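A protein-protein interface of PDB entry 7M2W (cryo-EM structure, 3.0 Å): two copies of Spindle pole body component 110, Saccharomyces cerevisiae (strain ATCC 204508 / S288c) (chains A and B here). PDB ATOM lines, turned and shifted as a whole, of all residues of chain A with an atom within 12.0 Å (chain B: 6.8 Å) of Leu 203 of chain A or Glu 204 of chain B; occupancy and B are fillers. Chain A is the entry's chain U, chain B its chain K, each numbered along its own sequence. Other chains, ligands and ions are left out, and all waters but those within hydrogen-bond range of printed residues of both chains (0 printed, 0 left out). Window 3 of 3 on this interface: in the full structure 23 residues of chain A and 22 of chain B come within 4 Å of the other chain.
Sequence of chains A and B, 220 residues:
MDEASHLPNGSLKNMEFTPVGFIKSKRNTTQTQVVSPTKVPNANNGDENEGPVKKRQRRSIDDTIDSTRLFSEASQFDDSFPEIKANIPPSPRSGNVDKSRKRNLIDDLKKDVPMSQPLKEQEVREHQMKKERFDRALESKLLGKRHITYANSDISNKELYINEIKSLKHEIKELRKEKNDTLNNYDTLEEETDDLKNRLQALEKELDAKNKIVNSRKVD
Leu 203 of chain A touches just these residues of chain B: Leu 200 (3.5 Å), Leu 203 (3.7 Å) and Glu 204 (3.7 Å). Of chain A, only Arg 199 and Leu 203 come within 4 Å of Glu 204 of chain B. Leu 200 of chain B touches just these residues of chain A: Leu 196 (3.3 Å), Arg 199 (3.5 Å), Leu 200 (3.1 Å) and Leu 203 (3.5 Å). No residue of chain A comes within 4 Å of Ala 202 of chain B. Of the printed residues of chain A, Leu 203 of chain B touches Leu 200, Leu 203 and Glu 204. No residue of chain A comes within 4 Å of Lys 205 of chain B. No residue of chain A comes within 4 Å of Glu 206 of chain B. Of the printed residues of chain B, Leu 200 of chain A touches Arg 199 (3.4 Å), Leu 200 (3.1 Å) and Leu 203 (3.9 Å). Printed residues of chain B within 4 Å of Leu 196 of chain A: Leu 200 (3.3 Å). Asn 198 of chain A touches none of the printed residues of chain B. The nearest residue of chain B that does not touch Leu 203 of chain A is Arg 199 of chain B (5.1 Å). The nearest printed residue of chain A that does not touch Arg 199 of chain B is Leu 203 of chain A (5.1 Å).
Leu 196 of chain A touches Leu 200 of chain B. Arg 199 of chain A touches Leu 200 of chain B. Leu 200 of chain A touches Arg 199 of chain B. Leu 200 of chain A touches Leu 200 of chain B (N to CD2, 3.1 Å). CD1 of Leu 200 of chain A touches CD1 of Leu 203 of chain B (3.9 Å). Leu 200 of chain B touches Leu 203 of chain A (O to CD1, 3.5 Å). Leu 203 of chain A touches Leu 203 of chain B. CA of Glu 204 of chain B touches CD2 of Leu 203 of chain A, at 3.7 Å. Glu 204 of chain A touches Leu 203 of chain B (CG to CD1, 3.5 Å).
Arg 199 of chain A touches Leu 200 of chain B, and with the chains exchanged Leu 200 of chain A touches Arg 199 of chain B. Arg 199 of chain A touches Glu 204 of chain B, and with the chains exchanged Glu 204 of chain A touches Arg 199 of chain B. Leu 200 of chain A touches its own counterpart, Leu 200 of chain B. Leu 203 of chain A touches Glu 204 of chain B, and with the chains exchanged Glu 204 of chain A touches Leu 203 of chain B. 7 positions are printed for both chains. Of the 11 pairs that touch across the chains among the printed residues, 10 have their exchanged pair printed and touching as well.
Hydrophobic or aromatic side chains of chain B within 4 Å of the printed part of chain A: Leu 200 and Leu 203. Printed residues of chain A that touch a printed residue of chain B: Leu 196, Arg 199, Leu 200, Leu 203 and Glu 204. Hydrophobic or aromatic side chains of chain A within 4 Å of the printed part of chain B: Leu 196, Leu 200 and Leu 203. Among the printed residues, 11 pairs touch across the chains.
The guanidinium group (NH2) of Arg 199 of chain B lies within salt-bridge range of the side-chain carboxylate (OE2) of Glu 204 of chain A (3.2 Å). The side-chain carboxylate of Glu 204 of chain B lies within salt-bridge range of the guanidinium group of Arg 199 of chain A (3.0 Å).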
ATOM      1  N   GLU A 192      18.394  15.271  10.214  1.00  0.00           N
ATOM      2  CA  GLU A 192      17.572  15.009  11.396  1.00  0.00           C
ATOM      3  C   GLU A 192      16.869  16.288  11.823  1.00  0.00           C
ATOM      4  O   GLU A 192      15.675  16.277  12.152  1.00  0.00           O
ATOM      5  CB  GLU A 192      18.401  14.487  12.576  1.00  0.00           C
ATOM      6  CG  GLU A 192      17.553  14.147  13.824  1.00  0.00           C
ATOM      7  CD  GLU A 192      18.350  13.581  14.983  1.00  0.00           C
ATOM      8  OE1 GLU A 192      19.541  13.475  14.875  1.00  0.00           O
ATOM      9  OE2 GLU A 192      17.744  13.245  15.986  1.00  0.00           O
ATOM     10  N   THR A 193      17.610  17.394  11.791  1.00  0.00           N
ATOM     11  CA  THR A 193      17.103  18.685  12.210  1.00  0.00           C
ATOM     12  C   THR A 193      15.894  19.066  11.366  1.00  0.00           C
ATOM     13  O   THR A 193      14.874  19.510  11.903  1.00  0.00           O
ATOM     14  CB  THR A 193      18.187  19.775  12.072  1.00  0.00           C
ATOM     15  OG1 THR A 193      19.318  19.439  12.873  1.00  0.00           O
ATOM     16  CG2 THR A 193      17.646  21.096  12.571  1.00  0.00           C
ATOM     17  N   ASP A 194      15.983  18.874  10.047  1.00  0.00           N
ATOM     18  CA  ASP A 194      14.869  19.223   9.180  1.00  0.00           C
ATOM     19  C   ASP A 194      13.656  18.334   9.406  1.00  0.00           C
ATOM     20  O   ASP A 194      12.527  18.834   9.401  1.00  0.00           O
ATOM     21  CB  ASP A 194      15.257  19.154   7.710  1.00  0.00           C
ATOM     22  CG  ASP A 194      16.154  20.300   7.235  1.00  0.00           C
ATOM     23  OD1 ASP A 194      16.304  21.276   7.927  1.00  0.00           O
ATOM     24  OD2 ASP A 194      16.630  20.197   6.115  1.00  0.00           O
ATOM     25  N   ASP A 195      13.854  17.037   9.669  1.00  0.00           N
ATOM     26  CA  ASP A 195      12.686  16.204   9.914  1.00  0.00           C
ATOM     27  C   ASP A 195      11.969  16.697  11.162  1.00  0.00           C
ATOM     28  O   ASP A 195      10.732  16.762  11.201  1.00  0.00           O
ATOM     29  CB  ASP A 195      13.069  14.737  10.133  1.00  0.00           C
ATOM     30  CG  ASP A 195      13.516  13.985   8.880  1.00  0.00           C
ATOM     31  OD1 ASP A 195      13.319  14.463   7.785  1.00  0.00           O
ATOM     32  OD2 ASP A 195      14.038  12.908   9.042  1.00  0.00           O
ATOM     33  N   LEU A 196      12.746  17.104  12.169  1.00  0.00           N
ATOM     34  CA  LEU A 196      12.156  17.595  13.398  1.00  0.00           C
ATOM     35  C   LEU A 196      11.414  18.893  13.131  1.00  0.00           C
ATOM     36  O   LEU A 196      10.313  19.090  13.650  1.00  0.00           O
ATOM     37  CB  LEU A 196      13.243  17.848  14.433  1.00  0.00           C
ATOM     38  CG  LEU A 196      14.007  16.639  14.964  1.00  0.00           C
ATOM     39  CD1 LEU A 196      15.152  17.156  15.768  1.00  0.00           C
ATOM     40  CD2 LEU A 196      13.141  15.762  15.817  1.00  0.00           C
ATOM     41  N   LYS A 197      11.979  19.764  12.284  1.00  0.00           N
ATOM     42  CA  LYS A 197      11.297  21.011  11.975  1.00  0.00           C
ATOM     43  C   LYS A 197       9.982  20.766  11.279  1.00  0.00           C
ATOM     44  O   LYS A 197       8.998  21.434  11.589  1.00  0.00           O
ATOM     45  CB  LYS A 197      12.127  21.933  11.083  1.00  0.00           C
ATOM     46  CG  LYS A 197      13.291  22.552  11.760  1.00  0.00           C
ATOM     47  CD  LYS A 197      14.070  23.480  10.857  1.00  0.00           C
ATOM     48  CE  LYS A 197      15.168  24.144  11.651  1.00  0.00           C
ATOM     49  NZ  LYS A 197      15.998  25.080  10.853  1.00  0.00           N
ATOM     50  N   ASN A 198       9.941  19.797  10.372  1.00  0.00           N
ATOM     51  CA  ASN A 198       8.703  19.554   9.655  1.00  0.00           C
ATOM     52  C   ASN A 198       7.633  19.014  10.594  1.00  0.00           C
ATOM     53  O   ASN A 198       6.464  19.422  10.521  1.00  0.00           O
ATOM     54  CB  ASN A 198       8.967  18.589   8.527  1.00  0.00           C
ATOM     55  CG  ASN A 198       9.761  19.219   7.436  1.00  0.00           C
ATOM     56  OD1 ASN A 198       9.795  20.441   7.276  1.00  0.00           O
ATOM     57  ND2 ASN A 198      10.426  18.406   6.671  1.00  0.00           N
ATOM     58  N   ARG A 199       8.041  18.157  11.538  1.00  0.00           N
ATOM     59  CA  ARG A 199       7.104  17.614  12.502  1.00  0.00           C
ATOM     60  C   ARG A 199       6.578  18.724  13.392  1.00  0.00           C
ATOM     61  O   ARG A 199       5.381  18.785  13.692  1.00  0.00           O
ATOM     62  CB  ARG A 199       7.779  16.559  13.369  1.00  0.00           C
ATOM     63  CG  ARG A 199       8.095  15.251  12.688  1.00  0.00           C
ATOM     64  CD  ARG A 199       9.018  14.404  13.508  1.00  0.00           C
ATOM     65  NE  ARG A 199       8.446  14.008  14.804  1.00  0.00           N
ATOM     66  CZ  ARG A 199       9.147  13.399  15.791  1.00  0.00           C
ATOM     67  NH1 ARG A 199      10.424  13.110  15.610  1.00  0.00           N
ATOM     68  NH2 ARG A 199       8.564  13.090  16.946  1.00  0.00           N
ATOM     69  N   LEU A 200       7.468  19.639  13.762  1.00  0.00           N
ATOM     70  CA  LEU A 200       7.099  20.712  14.648  1.00  0.00           C
ATOM     71  C   LEU A 200       6.180  21.682  13.958  1.00  0.00           C
ATOM     72  O   LEU A 200       5.181  22.095  14.545  1.00  0.00           O
ATOM     73  CB  LEU A 200       8.350  21.426  15.164  1.00  0.00           C
ATOM     74  CG  LEU A 200       8.147  22.511  16.218  1.00  0.00           C
ATOM     75  CD1 LEU A 200       7.422  21.946  17.459  1.00  0.00           C
ATOM     76  CD2 LEU A 200       9.494  23.015  16.621  1.00  0.00           C
ATOM     77  N   GLN A 201       6.434  21.980  12.688  1.00  0.00           N
ATOM     78  CA  GLN A 201       5.573  22.902  11.982  1.00  0.00           C
ATOM     79  C   GLN A 201       4.167  22.335  11.930  1.00  0.00           C
ATOM     80  O   GLN A 201       3.195  23.076  12.074  1.00  0.00           O
ATOM     81  CB  GLN A 201       6.112  23.132  10.578  1.00  0.00           C
ATOM     82  CG  GLN A 201       7.401  23.935  10.538  1.00  0.00           C
ATOM     83  CD  GLN A 201       8.013  23.948   9.165  1.00  0.00           C
ATOM     84  OE1 GLN A 201       7.640  23.133   8.316  1.00  0.00           O
ATOM     85  NE2 GLN A 201       8.950  24.860   8.932  1.00  0.00           N
ATOM     86  N   ALA A 202       4.044  21.014  11.747  1.00  0.00           N
ATOM     87  CA  ALA A 202       2.723  20.403  11.757  1.00  0.00           C
ATOM     88  C   ALA A 202       2.052  20.524  13.138  1.00  0.00           C
ATOM     89  O   ALA A 202       0.845  20.782  13.226  1.00  0.00           O
ATOM     90  CB  ALA A 202       2.831  18.942  11.367  1.00  0.00           C
ATOM     91  N   LEU A 203       2.838  20.362  14.212  1.00  0.00           N
ATOM     92  CA  LEU A 203       2.343  20.436  15.593  1.00  0.00           C
ATOM     93  C   LEU A 203       1.967  21.847  16.047  1.00  0.00           C
ATOM     94  O   LEU A 203       0.989  22.036  16.771  1.00  0.00           O
ATOM     95  CB  LEU A 203       3.400  19.864  16.540  1.00  0.00           C
ATOM     96  CG  LEU A 203       3.668  18.340  16.455  1.00  0.00           C
ATOM     97  CD1 LEU A 203       4.913  18.023  17.241  1.00  0.00           C
ATOM     98  CD2 LEU A 203       2.488  17.554  17.045  1.00  0.00           C
ATOM     99  N   GLU A 204       2.704  22.846  15.579  1.00  0.00           N
ATOM    100  CA  GLU A 204       2.469  24.245  15.935  1.00  0.00           C
ATOM    101  C   GLU A 204       1.375  24.848  15.063  1.00  0.00           C
ATOM    102  O   GLU A 204       0.983  26.003  15.239  1.00  0.00           O
ATOM    103  CB  GLU A 204       3.751  25.096  15.798  1.00  0.00           C
ATOM    104  CG  GLU A 204       4.868  24.791  16.817  1.00  0.00           C
ATOM    105  CD  GLU A 204       6.142  25.637  16.642  1.00  0.00           C
ATOM    106  OE1 GLU A 204       6.245  26.335  15.662  1.00  0.00           O
ATOM    107  OE2 GLU A 204       6.992  25.596  17.517  1.00  0.00           O
ATOM    108  N   LYS A 205       0.911  24.070  14.097  1.00  0.00           N
ATOM    109  CA  LYS A 205      -0.089  24.496  13.142  1.00  0.00           C
ATOM    110  C   LYS A 205      -1.414  23.807  13.423  1.00  0.00           C
ATOM    111  O   LYS A 205      -2.475  24.295  13.029  1.00  0.00           O
ATOM    112  CB  LYS A 205       0.382  24.194  11.731  1.00  0.00           C
ATOM    113  N   ARG B 199      10.583  20.795  21.748  1.00  0.00           N
ATOM    114  CA  ARG B 199       9.443  21.547  21.262  1.00  0.00           C
ATOM    115  C   ARG B 199       8.396  20.630  20.652  1.00  0.00           C
ATOM    116  O   ARG B 199       7.204  20.932  20.718  1.00  0.00           O
ATOM    117  CB  ARG B 199       9.915  22.603  20.292  1.00  0.00           C
ATOM    118  CG  ARG B 199      10.673  23.736  20.974  1.00  0.00           C
ATOM    119  CD  ARG B 199      11.399  24.586  20.031  1.00  0.00           C
ATOM    120  NE  ARG B 199      10.515  25.249  19.104  1.00  0.00           N
ATOM    121  CZ  ARG B 199      10.915  26.031  18.090  1.00  0.00           C
ATOM    122  NH1 ARG B 199      12.212  26.279  17.912  1.00  0.00           N
ATOM    123  NH2 ARG B 199       9.998  26.551  17.273  1.00  0.00           N
ATOM    124  N   LEU B 200       8.837  19.530  20.033  1.00  0.00           N
ATOM    125  CA  LEU B 200       7.913  18.566  19.469  1.00  0.00           C
ATOM    126  C   LEU B 200       7.224  17.811  20.576  1.00  0.00           C
ATOM    127  O   LEU B 200       6.007  17.663  20.582  1.00  0.00           O
ATOM    128  CB  LEU B 200       8.661  17.494  18.660  1.00  0.00           C
ATOM    129  CG  LEU B 200       9.354  17.890  17.382  1.00  0.00           C
ATOM    130  CD1 LEU B 200      10.152  16.767  16.903  1.00  0.00           C
ATOM    131  CD2 LEU B 200       8.405  18.216  16.400  1.00  0.00           C
ATOM    132  N   GLN B 201       7.975  17.416  21.597  1.00  0.00           N
ATOM    133  CA  GLN B 201       7.393  16.608  22.659  1.00  0.00           C
ATOM    134  C   GLN B 201       6.300  17.369  23.377  1.00  0.00           C
ATOM    135  O   GLN B 201       5.223  16.833  23.655  1.00  0.00           O
ATOM    136  CB  GLN B 201       8.489  16.203  23.638  1.00  0.00           C
ATOM    137  CG  GLN B 201       9.481  15.200  23.060  1.00  0.00           C
ATOM    138  CD  GLN B 201      10.669  14.979  23.965  1.00  0.00           C
ATOM    139  OE1 GLN B 201      10.900  15.768  24.885  1.00  0.00           O
ATOM    140  NE2 GLN B 201      11.421  13.916  23.712  1.00  0.00           N
ATOM    141  N   ALA B 202       6.525  18.665  23.545  1.00  0.00           N
ATOM    142  CA  ALA B 202       5.599  19.563  24.207  1.00  0.00           C
ATOM    143  C   ALA B 202       4.229  19.618  23.528  1.00  0.00           C
ATOM    144  O   ALA B 202       3.245  20.012  24.158  1.00  0.00           O
ATOM    145  CB  ALA B 202       6.190  20.958  24.239  1.00  0.00           C
ATOM    146  N   LEU B 203       4.180  19.364  22.225  1.00  0.00           N
ATOM    147  CA  LEU B 203       2.931  19.445  21.491  1.00  0.00           C
ATOM    148  C   LEU B 203       2.381  18.083  21.080  1.00  0.00           C
ATOM    149  O   LEU B 203       1.162  17.894  21.003  1.00  0.00           O
ATOM    150  CB  LEU B 203       3.157  20.293  20.249  1.00  0.00           C
ATOM    151  CG  LEU B 203       3.628  21.739  20.482  1.00  0.00           C
ATOM    152  CD1 LEU B 203       3.885  22.368  19.154  1.00  0.00           C
ATOM    153  CD2 LEU B 203       2.580  22.538  21.259  1.00  0.00           C
ATOM    154  N   GLU B 204       3.280  17.140  20.790  1.00  0.00           N
ATOM    155  CA  GLU B 204       2.904  15.822  20.310  1.00  0.00           C
ATOM    156  C   GLU B 204       2.332  14.961  21.419  1.00  0.00           C
ATOM    157  O   GLU B 204       1.341  14.251  21.218  1.00  0.00           O
ATOM    158  CB  GLU B 204       4.101  15.123  19.669  1.00  0.00           C
ATOM    159  CG  GLU B 204       3.771  13.810  18.993  1.00  0.00           C
ATOM    160  CD  GLU B 204       4.922  13.259  18.200  1.00  0.00           C
ATOM    161  OE1 GLU B 204       5.965  13.868  18.184  1.00  0.00           O
ATOM    162  OE2 GLU B 204       4.760  12.230  17.601  1.00  0.00           O
ATOM    163  N   LYS B 205       2.913  15.028  22.618  1.00  0.00           N
ATOM    164  CA  LYS B 205       2.437  14.203  23.719  1.00  0.00           C
ATOM    165  C   LYS B 205       1.247  14.889  24.366  1.00  0.00           C
ATOM    166  O   LYS B 205       1.291  15.310  25.522  1.00  0.00           O
ATOM    167  CB  LYS B 205       3.546  13.989  24.729  1.00  0.00           C
ATOM    168  N   GLU B 206       0.182  14.989  23.590  1.00  0.00           N
ATOM    169  CA  GLU B 206      -1.005  15.719  23.972  1.00  0.00           C
ATOM    170  C   GLU B 206      -2.127  15.459  22.983  1.00  0.00           C
ATOM    171  O   GLU B 206      -3.296  15.719  23.274  1.00  0.00           O
ATOM    172  CB  GLU B 206      -0.683  17.207  24.033  1.00  0.00           C
